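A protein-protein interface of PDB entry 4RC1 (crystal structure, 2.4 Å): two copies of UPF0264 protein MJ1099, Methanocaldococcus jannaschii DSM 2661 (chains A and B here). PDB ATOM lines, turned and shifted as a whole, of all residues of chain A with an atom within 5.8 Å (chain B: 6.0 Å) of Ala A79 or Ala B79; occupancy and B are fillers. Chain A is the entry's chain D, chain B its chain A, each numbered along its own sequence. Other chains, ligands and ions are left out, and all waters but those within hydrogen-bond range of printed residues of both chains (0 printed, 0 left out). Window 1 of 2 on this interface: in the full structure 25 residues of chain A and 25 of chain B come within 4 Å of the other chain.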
ATOM      1  N   VAL A  66      28.410   8.878  21.653  1.00  0.00           N
ATOM      2  CA  VAL A  66      28.532   7.921  20.529  1.00  0.00           C
ATOM      3  C   VAL A  66      28.893   8.677  19.211  1.00  0.00           C
ATOM      4  O   VAL A  66      29.158   8.049  18.192  1.00  0.00           O
ATOM      5  CB  VAL A  66      27.353   6.911  20.366  1.00  0.00           C
ATOM      6  CG1 VAL A  66      27.262   5.958  21.555  1.00  0.00           C
ATOM      7  CG2 VAL A  66      26.027   7.626  20.116  1.00  0.00           C
ATOM      8  N   GLY A  74      20.933   1.742  12.798  1.00  0.00           N
ATOM      9  CA  GLY A  74      21.640   0.482  13.036  1.00  0.00           C
ATOM     10  C   GLY A  74      23.028   0.660  13.617  1.00  0.00           C
ATOM     11  O   GLY A  74      23.356   0.062  14.640  1.00  0.00           O
ATOM     12  N   THR A  75      23.831   1.506  12.990  1.00  0.00           N
ATOM     13  CA  THR A  75      25.198   1.818  13.412  1.00  0.00           C
ATOM     14  C   THR A  75      25.227   2.450  14.811  1.00  0.00           C
ATOM     15  O   THR A  75      26.040   2.066  15.649  1.00  0.00           O
ATOM     16  CB  THR A  75      25.889   2.742  12.358  1.00  0.00           C
ATOM     17  OG1 THR A  75      25.942   2.073  11.104  1.00  0.00           O
ATOM     18  CG2 THR A  75      27.305   3.148  12.756  1.00  0.00           C
ATOM     19  N   ILE A  76      24.330   3.414  15.052  1.00  0.00           N
ATOM     20  CA  ILE A  76      24.254   4.154  16.304  1.00  0.00           C
ATOM     21  C   ILE A  76      23.734   3.304  17.453  1.00  0.00           C
ATOM     22  O   ILE A  76      24.207   3.463  18.573  1.00  0.00           O
ATOM     23  CB  ILE A  76      23.590   5.561  16.102  1.00  0.00           C
ATOM     24  CG1 ILE A  76      24.238   6.331  14.892  1.00  0.00           C
ATOM     25  CG2 ILE A  76      23.615   6.408  17.370  1.00  0.00           C
ATOM     26  CD1 ILE A  76      25.841   6.410  14.825  1.00  0.00           C
ATOM     27  N   SER A  77      22.822   2.347  17.157  1.00  0.00           N
ATOM     28  CA  SER A  77      22.291   1.390  18.131  1.00  0.00           C
ATOM     29  C   SER A  77      23.409   0.485  18.573  1.00  0.00           C
ATOM     30  O   SER A  77      23.561   0.257  19.773  1.00  0.00           O
ATOM     31  CB  SER A  77      21.149   0.569  17.540  1.00  0.00           C
ATOM     32  OG  SER A  77      20.052   1.420  17.270  1.00  0.00           O
ATOM     33  N   LEU A  78      24.220   0.003  17.611  1.00  0.00           N
ATOM     34  CA  LEU A  78      25.390  -0.849  17.869  1.00  0.00           C
ATOM     35  C   LEU A  78      26.447  -0.098  18.679  1.00  0.00           C
ATOM     36  O   LEU A  78      26.965  -0.651  19.640  1.00  0.00           O
ATOM     37  CB  LEU A  78      25.985  -1.395  16.564  1.00  0.00           C
ATOM     38  CG  LEU A  78      25.142  -2.433  15.806  1.00  0.00           C
ATOM     39  CD1 LEU A  78      25.766  -2.733  14.450  1.00  0.00           C
ATOM     40  CD2 LEU A  78      24.883  -3.706  16.643  1.00  0.00           C
ATOM     41  N   ALA A  79      26.706   1.173  18.335  1.00  0.00           N
ATOM     42  CA  ALA A  79      27.652   2.046  19.046  1.00  0.00           C
ATOM     43  C   ALA A  79      27.213   2.300  20.488  1.00  0.00           C
ATOM     44  O   ALA A  79      28.052   2.318  21.392  1.00  0.00           O
ATOM     45  CB  ALA A  79      27.856   3.371  18.283  1.00  0.00           C
ATOM     46  N   ALA A  80      25.898   2.448  20.707  1.00  0.00           N
ATOM     47  CA  ALA A  80      25.281   2.657  22.033  1.00  0.00           C
ATOM     48  C   ALA A  80      25.473   1.418  22.908  1.00  0.00           C
ATOM     49  O   ALA A  80      25.768   1.555  24.089  1.00  0.00           O
ATOM     50  CB  ALA A  80      23.801   3.006  21.884  1.00  0.00           C
ATOM     51  N   VAL A  81      25.380   0.200  22.308  1.00  0.00           N
ATOM     52  CA  VAL A  81      25.654  -1.098  22.955  1.00  0.00           C
ATOM     53  C   VAL A  81      27.154  -1.139  23.370  1.00  0.00           C
ATOM     54  O   VAL A  81      27.477  -1.489  24.504  1.00  0.00           O
ATOM     55  CB  VAL A  81      25.269  -2.304  22.055  1.00  0.00           C
ATOM     56  CG1 VAL A  81      25.802  -3.629  22.618  1.00  0.00           C
ATOM     57  CG2 VAL A  81      23.772  -2.375  21.863  1.00  0.00           C
ATOM     58  N   GLY A  82      28.026  -0.748  22.455  1.00  0.00           N
ATOM     59  CA  GLY A  82      29.457  -0.653  22.684  1.00  0.00           C
ATOM     60  C   GLY A  82      29.823   0.247  23.849  1.00  0.00           C
ATOM     61  O   GLY A  82      30.647  -0.144  24.675  1.00  0.00           O
ATOM     62  N   ALA A  83      29.195   1.453  23.942  1.00  0.00           N
ATOM     63  CA  ALA A  83      29.418   2.422  25.017  1.00  0.00           C
ATOM     64  C   ALA A  83      28.913   1.888  26.371  1.00  0.00           C
ATOM     65  O   ALA A  83      29.639   1.974  27.371  1.00  0.00           O
ATOM     66  CB  ALA A  83      28.751   3.751  24.682  1.00  0.00           C
ATOM     67  N   ALA A  84      27.687   1.304  26.388  1.00  0.00           N
ATOM     68  CA  ALA A  84      27.055   0.706  27.559  1.00  0.00           C
ATOM     69  C   ALA A  84      27.879  -0.486  28.115  1.00  0.00           C
ATOM     70  O   ALA A  84      28.171  -0.515  29.306  1.00  0.00           O
ATOM     71  CB  ALA A  84      25.636   0.274  27.219  1.00  0.00           C
ATOM     72  N   VAL B  66      28.796  -2.978  10.168  1.00  0.00           N
ATOM     73  CA  VAL B  66      28.670  -1.843  11.093  1.00  0.00           C
ATOM     74  C   VAL B  66      28.246  -0.582  10.307  1.00  0.00           C
ATOM     75  O   VAL B  66      27.960   0.455  10.894  1.00  0.00           O
ATOM     76  CB  VAL B  66      29.920  -1.640  12.016  1.00  0.00           C
ATOM     77  CG1 VAL B  66      30.097  -2.821  12.990  1.00  0.00           C
ATOM     78  CG2 VAL B  66      31.204  -1.395  11.215  1.00  0.00           C
ATOM     79  N   GLY B  74      36.143   6.319  16.670  1.00  0.00           N
ATOM     80  CA  GLY B  74      35.523   6.075  17.965  1.00  0.00           C
ATOM     81  C   GLY B  74      34.151   5.438  17.857  1.00  0.00           C
ATOM     82  O   GLY B  74      33.900   4.412  18.494  1.00  0.00           O
ATOM     83  N   THR B  75      33.262   6.025  17.031  1.00  0.00           N
ATOM     84  CA  THR B  75      31.895   5.541  16.787  1.00  0.00           C
ATOM     85  C   THR B  75      31.903   4.138  16.203  1.00  0.00           C
ATOM     86  O   THR B  75      31.146   3.292  16.640  1.00  0.00           O
ATOM     87  CB  THR B  75      31.150   6.541  15.843  1.00  0.00           C
ATOM     88  OG1 THR B  75      31.113   7.817  16.457  1.00  0.00           O
ATOM     89  CG2 THR B  75      29.725   6.099  15.496  1.00  0.00           C
ATOM     90  N   ILE B  76      32.742   3.905  15.192  1.00  0.00           N
ATOM     91  CA  ILE B  76      32.838   2.620  14.482  1.00  0.00           C
ATOM     92  C   ILE B  76      33.468   1.513  15.357  1.00  0.00           C
ATOM     93  O   ILE B  76      33.068   0.350  15.256  1.00  0.00           O
ATOM     94  CB  ILE B  76      33.457   2.816  13.062  1.00  0.00           C
ATOM     95  CG1 ILE B  76      32.767   3.974  12.281  1.00  0.00           C
ATOM     96  CG2 ILE B  76      33.450   1.492  12.249  1.00  0.00           C
ATOM     97  CD1 ILE B  76      31.113   4.011  12.222  1.00  0.00           C
ATOM     98  N   SER B  77      34.399   1.882  16.256  1.00  0.00           N
ATOM     99  CA  SER B  77      35.004   0.939  17.217  1.00  0.00           C
ATOM    100  C   SER B  77      33.918   0.493  18.216  1.00  0.00           C
ATOM    101  O   SER B  77      33.821  -0.691  18.523  1.00  0.00           O
ATOM    102  CB  SER B  77      36.151   1.589  17.983  1.00  0.00           C
ATOM    103  OG  SER B  77      37.206   1.889  17.096  1.00  0.00           O
ATOM    104  N   LEU B  78      33.095   1.444  18.684  1.00  0.00           N
ATOM    105  CA  LEU B  78      31.989   1.169  19.593  1.00  0.00           C
ATOM    106  C   LEU B  78      30.933   0.300  18.900  1.00  0.00           C
ATOM    107  O   LEU B  78      30.453  -0.652  19.496  1.00  0.00           O
ATOM    108  CB  LEU B  78      31.379   2.471  20.125  1.00  0.00           C
ATOM    109  CG  LEU B  78      32.235   3.325  21.100  1.00  0.00           C
ATOM    110  CD1 LEU B  78      31.572   4.668  21.350  1.00  0.00           C
ATOM    111  CD2 LEU B  78      32.459   2.610  22.434  1.00  0.00           C
ATOM    112  N   ALA B  79      30.606   0.596  17.637  1.00  0.00           N
ATOM    113  CA  ALA B  79      29.648  -0.172  16.822  1.00  0.00           C
ATOM    114  C   ALA B  79      30.140  -1.606  16.587  1.00  0.00           C
ATOM    115  O   ALA B  79      29.318  -2.528  16.614  1.00  0.00           O
ATOM    116  CB  ALA B  79      29.387   0.536  15.495  1.00  0.00           C
ATOM    117  N   ALA B  80      31.476  -1.811  16.415  1.00  0.00           N
ATOM    118  CA  ALA B  80      32.080  -3.153  16.241  1.00  0.00           C
ATOM    119  C   ALA B  80      31.979  -3.961  17.521  1.00  0.00           C
ATOM    120  O   ALA B  80      31.766  -5.170  17.446  1.00  0.00           O
ATOM    121  CB  ALA B  80      33.533  -3.058  15.787  1.00  0.00           C
ATOM    122  N   VAL B  81      32.099  -3.292  18.698  1.00  0.00           N
ATOM    123  CA  VAL B  81      31.919  -3.887  20.017  1.00  0.00           C
ATOM    124  C   VAL B  81      30.445  -4.337  20.121  1.00  0.00           C
ATOM    125  O   VAL B  81      30.188  -5.466  20.524  1.00  0.00           O
ATOM    126  CB  VAL B  81      32.327  -2.930  21.184  1.00  0.00           C
ATOM    127  CG1 VAL B  81      31.884  -3.476  22.536  1.00  0.00           C
ATOM    128  CG2 VAL B  81      33.818  -2.682  21.198  1.00  0.00           C
ATOM    129  N   GLY B  82      29.515  -3.462  19.734  1.00  0.00           N
ATOM    130  CA  GLY B  82      28.082  -3.733  19.723  1.00  0.00           C
ATOM    131  C   GLY B  82      27.692  -4.929  18.877  1.00  0.00           C
ATOM    132  O   GLY B  82      26.901  -5.753  19.323  1.00  0.00           O
ATOM    133  N   ALA B  83      28.269  -5.050  17.660  1.00  0.00           N
ATOM    134  CA  ALA B  83      28.063  -6.174  16.742  1.00  0.00           C
ATOM    135  C   ALA B  83      28.676  -7.480  17.326  1.00  0.00           C
ATOM    136  O   ALA B  83      28.012  -8.514  17.296  1.00  0.00           O
ATOM    137  CB  ALA B  83      28.666  -5.870  15.380  1.00  0.00           C
ATOM    138  N   ALA B  84      29.900  -7.410  17.907  1.00  0.00           N
ATOM    139  CA  ALA B  84      30.609  -8.555  18.491  1.00  0.00           C
ATOM    140  C   ALA B  84      29.878  -9.100  19.708  1.00  0.00           C
ATOM    141  O   ALA B  84      29.693 -10.310  19.802  1.00  0.00           O
ATOM    142  CB  ALA B  84      32.032  -8.166  18.867  1.00  0.00           C
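Of the printed residues of chain B, Val A66 touches Thr B75 (2.6 Å).
Of the printed residues of chain B, Thr A75 touches Val B66 (2.6 Å), Ile B76 (3.9 Å) and Ala B79 (3.7 Å).
Of the printed residues of chain B, Leu A78 touches Leu B78 (3.5 Å), Ala B79 (3.5 Å), Gly B82 (3.3 Å) and Ala B83 (3.8 Å).
Gly B74 touches none of the printed residues of chain A.
Ala B79 touches just these residues of chain A: Thr A75, Leu A78 and Ala A79.
Of the printed residues of chain A, Ala B83 touches Leu A78 (3.8 Å).
The backbone carbonyl oxygen (O) of Val B66 lies within hydrogen-bond range of the side-chain hydroxyl (OG1) of Thr A75 (2.6 Å).
The side-chain hydroxyl (OG1) of Thr B75 lies within hydrogen-bond range of the backbone carbonyl oxygen (O) of Val A66, at 2.6 Å.
O of Leu A78 sits close to O of Leu B78.
Ile B76 touches Thr A75 (CD1 to CG2, 3.9 Å).
CB of Ala B79 touches O of Thr A75 (3.7 Å).
Thr B75 touches Ile A76 (CG2 to CD1, 3.95 Å).
CB of Leu A78 touches O of Ala B79, at 3.5 Å.
Leu A78 touches Gly B82.
Ala B83 touches Leu A78 (N to CD2, 3.8 Å).
CB of Ala A79 touches O of Thr B75, 3.7 Å away.
N of Ala A79 touches CA of Ala B79 (3.6 Å).
Leu B78 touches Gly A82 (O to CA, 3.3 Å).
Gly A82 touches Val B81.
Hydrophobic or aromatic side chains of chain A within 4 Å of the printed part of chain B: Ile A76, Leu A78, Ala A79 and Val A81.
Of the 12 printed residues of chain B, 8 touch a printed residue of chain A.
Hydrophobic or aromatic side chains of chain B within 4 Å of the printed part of chain A: Ile B76, Leu B78, Ala B79 and Val B81.
Among the printed residues, 16 pairs touch across the chains.
Leu A78 touches its own counterpart, Leu B78.
Leu A78 touches Gly B82, and with the chains exchanged Gly A82 touches Leu B78.
Leu A78 touches Ala B83, and with the chains exchanged Ala A83 touches Leu B78.
Val A81 touches Gly B82, and with the chains exchanged Gly A82 touches Val B81.
12 positions are printed for both chains.
Of the 16 pairs that touch across the chains among the printed residues, 16 have their exchanged pair printed and touching as well.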
